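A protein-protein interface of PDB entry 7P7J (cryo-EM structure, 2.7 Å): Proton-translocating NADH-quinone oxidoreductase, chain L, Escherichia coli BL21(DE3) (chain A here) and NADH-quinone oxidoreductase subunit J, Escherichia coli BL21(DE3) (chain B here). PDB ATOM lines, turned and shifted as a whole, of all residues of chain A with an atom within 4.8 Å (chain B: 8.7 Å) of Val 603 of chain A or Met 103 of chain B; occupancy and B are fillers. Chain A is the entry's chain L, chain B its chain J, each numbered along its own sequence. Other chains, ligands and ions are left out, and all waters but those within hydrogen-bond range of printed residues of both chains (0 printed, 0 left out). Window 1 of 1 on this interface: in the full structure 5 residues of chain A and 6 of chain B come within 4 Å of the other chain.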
ATOM      1  N   SER A 599      -8.190  17.073  10.368  1.00  0.00           N
ATOM      2  CA  SER A 599      -9.637  17.268  10.448  1.00  0.00           C
ATOM      3  C   SER A 599     -10.255  16.468  11.594  1.00  0.00           C
ATOM      4  O   SER A 599     -11.203  16.934  12.237  1.00  0.00           O
ATOM      5  CB  SER A 599     -10.292  16.899   9.120  1.00  0.00           C
ATOM      6  OG  SER A 599      -9.827  15.651   8.652  1.00  0.00           O
ATOM      7  N   ILE A 600      -9.732  15.269  11.866  1.00  0.00           N
ATOM      8  CA  ILE A 600     -10.193  14.471  13.003  1.00  0.00           C
ATOM      9  C   ILE A 600      -9.908  15.199  14.310  1.00  0.00           C
ATOM     10  O   ILE A 600     -10.760  15.261  15.206  1.00  0.00           O
ATOM     11  CB  ILE A 600      -9.535  13.077  12.973  1.00  0.00           C
ATOM     12  CG1 ILE A 600     -10.251  12.158  11.987  1.00  0.00           C
ATOM     13  CG2 ILE A 600      -9.526  12.429  14.350  1.00  0.00           C
ATOM     14  CD1 ILE A 600      -9.577  10.820  11.811  1.00  0.00           C
ATOM     15  N   GLY A 601      -8.709  15.774  14.431  1.00  0.00           N
ATOM     16  CA  GLY A 601      -8.388  16.572  15.597  1.00  0.00           C
ATOM     17  C   GLY A 601      -9.232  17.821  15.714  1.00  0.00           C
ATOM     18  O   GLY A 601      -9.564  18.243  16.822  1.00  0.00           O
ATOM     19  N   ALA A 602      -9.587  18.430  14.580  1.00  0.00           N
ATOM     20  CA  ALA A 602     -10.507  19.561  14.602  1.00  0.00           C
ATOM     21  C   ALA A 602     -11.874  19.151  15.131  1.00  0.00           C
ATOM     22  O   ALA A 602     -12.473  19.864  15.944  1.00  0.00           O
ATOM     23  CB  ALA A 602     -10.630  20.162  13.203  1.00  0.00           C
ATOM     24  N   VAL A 603     -12.365  17.987  14.696  1.00  0.00           N
ATOM     25  CA  VAL A 603     -13.639  17.462  15.184  1.00  0.00           C
ATOM     26  C   VAL A 603     -13.569  17.196  16.682  1.00  0.00           C
ATOM     27  O   VAL A 603     -14.489  17.543  17.431  1.00  0.00           O
ATOM     28  CB  VAL A 603     -14.019  16.192  14.401  1.00  0.00           C
ATOM     29  CG1 VAL A 603     -15.166  15.455  15.072  1.00  0.00           C
ATOM     30  CG2 VAL A 603     -14.380  16.540  12.980  1.00  0.00           C
ATOM     31  N   VAL A 604     -12.467  16.599  17.141  1.00  0.00           N
ATOM     32  CA  VAL A 604     -12.317  16.262  18.554  1.00  0.00           C
ATOM     33  C   VAL A 604     -12.236  17.523  19.410  1.00  0.00           C
ATOM     34  O   VAL A 604     -12.884  17.614  20.460  1.00  0.00           O
ATOM     35  CB  VAL A 604     -11.092  15.351  18.751  1.00  0.00           C
ATOM     36  CG1 VAL A 604     -10.702  15.260  20.216  1.00  0.00           C
ATOM     37  CG2 VAL A 604     -11.377  13.967  18.199  1.00  0.00           C
ATOM     38  N   VAL A 605     -11.462  18.520  18.969  1.00  0.00           N
ATOM     39  CA  VAL A 605     -11.327  19.768  19.718  1.00  0.00           C
ATOM     40  C   VAL A 605     -12.658  20.510  19.773  1.00  0.00           C
ATOM     41  O   VAL A 605     -13.065  21.006  20.833  1.00  0.00           O
ATOM     42  CB  VAL A 605     -10.211  20.634  19.102  1.00  0.00           C
ATOM     43  CG1 VAL A 605     -10.322  22.081  19.554  1.00  0.00           C
ATOM     44  CG2 VAL A 605      -8.849  20.076  19.469  1.00  0.00           C
ATOM     45  N   LEU A 606     -13.370  20.573  18.642  1.00  0.00           N
ATOM     46  CA  LEU A 606     -14.665  21.243  18.613  1.00  0.00           C
ATOM     47  C   LEU A 606     -15.686  20.529  19.489  1.00  0.00           C
ATOM     48  O   LEU A 606     -16.447  21.179  20.213  1.00  0.00           O
ATOM     49  CB  LEU A 606     -15.166  21.341  17.174  1.00  0.00           C
ATOM     50  CG  LEU A 606     -14.530  22.431  16.315  1.00  0.00           C
ATOM     51  CD1 LEU A 606     -15.087  22.392  14.907  1.00  0.00           C
ATOM     52  CD2 LEU A 606     -14.754  23.788  16.942  1.00  0.00           C
ATOM     53  N   ALA A 607     -15.704  19.194  19.454  1.00  0.00           N
ATOM     54  CA  ALA A 607     -16.640  18.440  20.281  1.00  0.00           C
ATOM     55  C   ALA A 607     -16.322  18.590  21.763  1.00  0.00           C
ATOM     56  O   ALA A 607     -17.235  18.704  22.588  1.00  0.00           O
ATOM     57  CB  ALA A 607     -16.627  16.968  19.876  1.00  0.00           C
ATOM     58  N   PRO B  96     -14.508  10.087   5.182  1.00  0.00           N
ATOM     59  CA  PRO B  96     -14.347  11.550   5.184  1.00  0.00           C
ATOM     60  C   PRO B  96     -15.647  12.328   5.066  1.00  0.00           C
ATOM     61  O   PRO B  96     -15.744  13.419   5.639  1.00  0.00           O
ATOM     62  CB  PRO B  96     -13.433  11.795   3.979  1.00  0.00           C
ATOM     63  CG  PRO B  96     -12.628  10.562   3.885  1.00  0.00           C
ATOM     64  CD  PRO B  96     -13.539   9.440   4.280  1.00  0.00           C
ATOM     65  N   ALA B  97     -16.649  11.814   4.344  1.00  0.00           N
ATOM     66  CA  ALA B  97     -17.939  12.496   4.303  1.00  0.00           C
ATOM     67  C   ALA B  97     -18.614  12.478   5.667  1.00  0.00           C
ATOM     68  O   ALA B  97     -19.224  13.472   6.072  1.00  0.00           O
ATOM     69  CB  ALA B  97     -18.853  11.870   3.254  1.00  0.00           C
ATOM     70  N   ILE B  98     -18.507  11.358   6.387  1.00  0.00           N
ATOM     71  CA  ILE B  98     -19.038  11.280   7.746  1.00  0.00           C
ATOM     72  C   ILE B  98     -18.320  12.267   8.657  1.00  0.00           C
ATOM     73  O   ILE B  98     -18.952  12.975   9.451  1.00  0.00           O
ATOM     74  CB  ILE B  98     -18.937   9.833   8.270  1.00  0.00           C
ATOM     75  CG1 ILE B  98     -20.050   8.970   7.678  1.00  0.00           C
ATOM     76  CG2 ILE B  98     -18.987   9.781   9.789  1.00  0.00           C
ATOM     77  CD1 ILE B  98     -19.894   7.501   7.982  1.00  0.00           C
ATOM     78  N   LEU B  99     -16.992  12.347   8.536  1.00  0.00           N
ATOM     79  CA  LEU B  99     -16.215  13.266   9.364  1.00  0.00           C
ATOM     80  C   LEU B  99     -16.570  14.722   9.076  1.00  0.00           C
ATOM     81  O   LEU B  99     -16.744  15.526  10.005  1.00  0.00           O
ATOM     82  CB  LEU B  99     -14.728  13.024   9.135  1.00  0.00           C
ATOM     83  CG  LEU B  99     -13.761  13.798  10.019  1.00  0.00           C
ATOM     84  CD1 LEU B  99     -13.774  13.218  11.417  1.00  0.00           C
ATOM     85  CD2 LEU B  99     -12.376  13.738   9.421  1.00  0.00           C
ATOM     86  N   SER B 100     -16.698  15.074   7.795  1.00  0.00           N
ATOM     87  CA  SER B 100     -17.065  16.436   7.424  1.00  0.00           C
ATOM     88  C   SER B 100     -18.490  16.763   7.846  1.00  0.00           C
ATOM     89  O   SER B 100     -18.773  17.897   8.240  1.00  0.00           O
ATOM     90  CB  SER B 100     -16.894  16.637   5.921  1.00  0.00           C
ATOM     91  OG  SER B 100     -15.526  16.605   5.554  1.00  0.00           O
ATOM     92  N   ALA B 101     -19.398  15.785   7.775  1.00  0.00           N
ATOM     93  CA  ALA B 101     -20.763  16.001   8.239  1.00  0.00           C
ATOM     94  C   ALA B 101     -20.809  16.231   9.743  1.00  0.00           C
ATOM     95  O   ALA B 101     -21.563  17.086  10.219  1.00  0.00           O
ATOM     96  CB  ALA B 101     -21.642  14.814   7.851  1.00  0.00           C
ATOM     97  N   ILE B 102     -20.005  15.482  10.504  1.00  0.00           N
ATOM     98  CA  ILE B 102     -19.948  15.672  11.953  1.00  0.00           C
ATOM     99  C   ILE B 102     -19.404  17.055  12.292  1.00  0.00           C
ATOM    100  O   ILE B 102     -19.953  17.764  13.150  1.00  0.00           O
ATOM    101  CB  ILE B 102     -19.111  14.554  12.603  1.00  0.00           C
ATOM    102  CG1 ILE B 102     -19.860  13.224  12.548  1.00  0.00           C
ATOM    103  CG2 ILE B 102     -18.768  14.891  14.045  1.00  0.00           C
ATOM    104  CD1 ILE B 102     -19.034  12.041  12.998  1.00  0.00           C
ATOM    105  N   MET B 103     -18.330  17.470  11.612  1.00  0.00           N
ATOM    106  CA  MET B 103     -17.766  18.792  11.869  1.00  0.00           C
ATOM    107  C   MET B 103     -18.724  19.902  11.451  1.00  0.00           C
ATOM    108  O   MET B 103     -18.834  20.922  12.141  1.00  0.00           O
ATOM    109  CB  MET B 103     -16.422  18.936  11.162  1.00  0.00           C
ATOM    110  CG  MET B 103     -15.783  20.308  11.290  1.00  0.00           C
ATOM    111  SD  MET B 103     -14.513  20.558  10.046  1.00  0.00           S
ATOM    112  CE  MET B 103     -13.663  18.988  10.181  1.00  0.00           C
ATOM    113  N   LEU B 104     -19.434  19.714  10.337  1.00  0.00           N
ATOM    114  CA  LEU B 104     -20.438  20.681   9.911  1.00  0.00           C
ATOM    115  C   LEU B 104     -21.572  20.779  10.920  1.00  0.00           C
ATOM    116  O   LEU B 104     -22.064  21.875  11.198  1.00  0.00           O
ATOM    117  CB  LEU B 104     -20.976  20.298   8.533  1.00  0.00           C
ATOM    118  CG  LEU B 104     -22.114  21.143   7.962  1.00  0.00           C
ATOM    119  CD1 LEU B 104     -21.680  22.588   7.812  1.00  0.00           C
ATOM    120  CD2 LEU B 104     -22.583  20.579   6.635  1.00  0.00           C
ATOM    121  N   VAL B 105     -21.990  19.644  11.487  1.00  0.00           N
ATOM    122  CA  VAL B 105     -23.038  19.647  12.503  1.00  0.00           C
ATOM    123  C   VAL B 105     -22.581  20.407  13.743  1.00  0.00           C
ATOM    124  O   VAL B 105     -23.328  21.224  14.297  1.00  0.00           O
ATOM    125  CB  VAL B 105     -23.456  18.200  12.832  1.00  0.00           C
ATOM    126  CG1 VAL B 105     -24.096  18.105  14.208  1.00  0.00           C
ATOM    127  CG2 VAL B 105     -24.408  17.677  11.771  1.00  0.00           C
ATOM    128  N   VAL B 106     -21.337  20.178  14.174  1.00  0.00           N
ATOM    129  CA  VAL B 106     -20.816  20.866  15.357  1.00  0.00           C
ATOM    130  C   VAL B 106     -20.703  22.370  15.112  1.00  0.00           C
ATOM    131  O   VAL B 106     -21.106  23.184  15.957  1.00  0.00           O
ATOM    132  CB  VAL B 106     -19.468  20.251  15.775  1.00  0.00           C
ATOM    133  CG1 VAL B 106     -18.825  21.072  16.872  1.00  0.00           C
ATOM    134  CG2 VAL B 106     -19.665  18.824  16.244  1.00  0.00           C
ATOM    135  N   ILE B 107     -20.183  22.765  13.947  1.00  0.00           N
ATOM    136  CA  ILE B 107     -20.019  24.183  13.636  1.00  0.00           C
ATOM    137  C   ILE B 107     -21.376  24.865  13.480  1.00  0.00           C
ATOM    138  O   ILE B 107     -21.569  25.997  13.936  1.00  0.00           O
ATOM    139  CB  ILE B 107     -19.137  24.347  12.383  1.00  0.00           C
ATOM    140  CG1 ILE B 107     -17.700  23.933  12.695  1.00  0.00           C
ATOM    141  CG2 ILE B 107     -19.140  25.780  11.885  1.00  0.00           C
ATOM    142  CD1 ILE B 107     -16.789  23.937  11.491  1.00  0.00           C
ATOM    143  N   VAL B 108     -22.346  24.180  12.868  1.00  0.00           N
ATOM    144  CA  VAL B 108     -23.685  24.739  12.717  1.00  0.00           C
ATOM    145  C   VAL B 108     -24.366  24.887  14.074  1.00  0.00           C
ATOM    146  O   VAL B 108     -25.044  25.889  14.333  1.00  0.00           O
ATOM    147  CB  VAL B 108     -24.504  23.871  11.739  1.00  0.00           C
ATOM    148  CG1 VAL B 108     -26.003  24.021  11.962  1.00  0.00           C
ATOM    149  CG2 VAL B 108     -24.156  24.233  10.306  1.00  0.00           C
ATOM    150  N   TYR B 109     -24.171  23.914  14.971  1.00  0.00           N
ATOM    151  CA  TYR B 109     -24.754  24.018  16.306  1.00  0.00           C
ATOM    152  C   TYR B 109     -24.132  25.180  17.070  1.00  0.00           C
ATOM    153  O   TYR B 109     -24.819  25.866  17.835  1.00  0.00           O
ATOM    154  CB  TYR B 109     -24.608  22.667  17.040  1.00  0.00           C
ATOM    155  CG  TYR B 109     -24.797  22.614  18.565  1.00  0.00           C
ATOM    156  CD1 TYR B 109     -23.867  23.147  19.462  1.00  0.00           C
ATOM    157  CD2 TYR B 109     -25.946  22.043  19.099  1.00  0.00           C
ATOM    158  CE1 TYR B 109     -24.073  23.096  20.826  1.00  0.00           C
ATOM    159  CE2 TYR B 109     -26.156  21.988  20.464  1.00  0.00           C
ATOM    160  CZ  TYR B 109     -25.217  22.515  21.320  1.00  0.00           C
ATOM    161  OH  TYR B 109     -25.421  22.462  22.679  1.00  0.00           O
ATOM    162  N   ALA B 110     -22.831  25.408  16.884  1.00  0.00           N
ATOM    163  CA  ALA B 110     -22.205  26.579  17.488  1.00  0.00           C
ATOM    164  C   ALA B 110     -22.717  27.877  16.872  1.00  0.00           C
ATOM    165  O   ALA B 110     -22.834  28.889  17.572  1.00  0.00           O
ATOM    166  CB  ALA B 110     -20.689  26.492  17.352  1.00  0.00           C
ATOM    167  N   ILE B 111     -23.008  27.865  15.570  1.00  0.00           N
ATOM    168  CA  ILE B 111     -23.513  29.053  14.887  1.00  0.00           C
ATOM    169  C   ILE B 111     -24.905  29.415  15.390  1.00  0.00           C
ATOM    170  O   ILE B 111     -25.198  30.587  15.659  1.00  0.00           O
ATOM    171  CB  ILE B 111     -23.495  28.823  13.363  1.00  0.00           C
ATOM    172  CG1 ILE B 111     -22.091  29.040  12.805  1.00  0.00           C
ATOM    173  CG2 ILE B 111     -24.483  29.734  12.649  1.00  0.00           C
ATOM    174  CD1 ILE B 111     -21.876  28.399  11.459  1.00  0.00           C
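Among the printed residues, merely in contact across the chains: Ser 599 of chain A with Leu 99 of chain B (3.3 Å), Ser 599 of chain A with Met 103 of chain B (3.8 Å), Ile 600 of chain A with Leu 99 of chain B (3.7 Å), Val 603 of chain A with Leu 99 of chain B (3.7 Å), Val 603 of chain A with Ile 102 of chain B (3.8 Å), Val 603 of chain A with Met 103 of chain B (3.6 Å), Leu 606 of chain A with Val 106 of chain B (3.7 Å) and Leu 606 of chain A with Ile 107 of chain B (3.8 Å).
Printed residues of chain B within 4 Å of Ile 600 of chain A: Leu 99 (3.7 Å). No residue of chain B comes within 4 Å of Gly 601 of chain A. No residue of chain B comes within 4 Å of Ala 602 of chain A. Val 603 of chain A touches three residues of chain B. Val 604 of chain A touches none of the printed residues of chain B. Printed residues of chain B within 4 Å of Leu 606 of chain A: Val 106 and Ile 107. Of the printed residues of chain A, Leu 99 of chain B touches Ser 599, Ile 600 and Val 603. Of chain A, only Ser 599 (3.8 Å) and Val 603 (3.6 Å) come within 4 Å of Met 103 of chain B. Of the printed residues of chain A, Val 106 of chain B touches Leu 606. Ala 110 of chain B touches none of the printed residues of chain A. The nearest residue of chain B that does not touch Val 603 of chain A is Val 106 of chain B (5.5 Å).
Of the 9 printed residues of chain A, 4 touch a printed residue of chain B. Hydrophobic or aromatic side chains of chain A that line the printed part of chain B: Ile 600, Val 603 and Leu 606. Of the 16 printed residues of chain B, 5 touch a printed residue of chain A. Hydrophobic or aromatic side chains of chain B that line the printed part of chain A: Leu 99, Ile 102, Met 103, Val 106 and Ile 107. Among the printed residues, no Asp or Glu carboxylate lies within 4 Å of a Lys or Arg side-chain nitrogen of the other chain.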
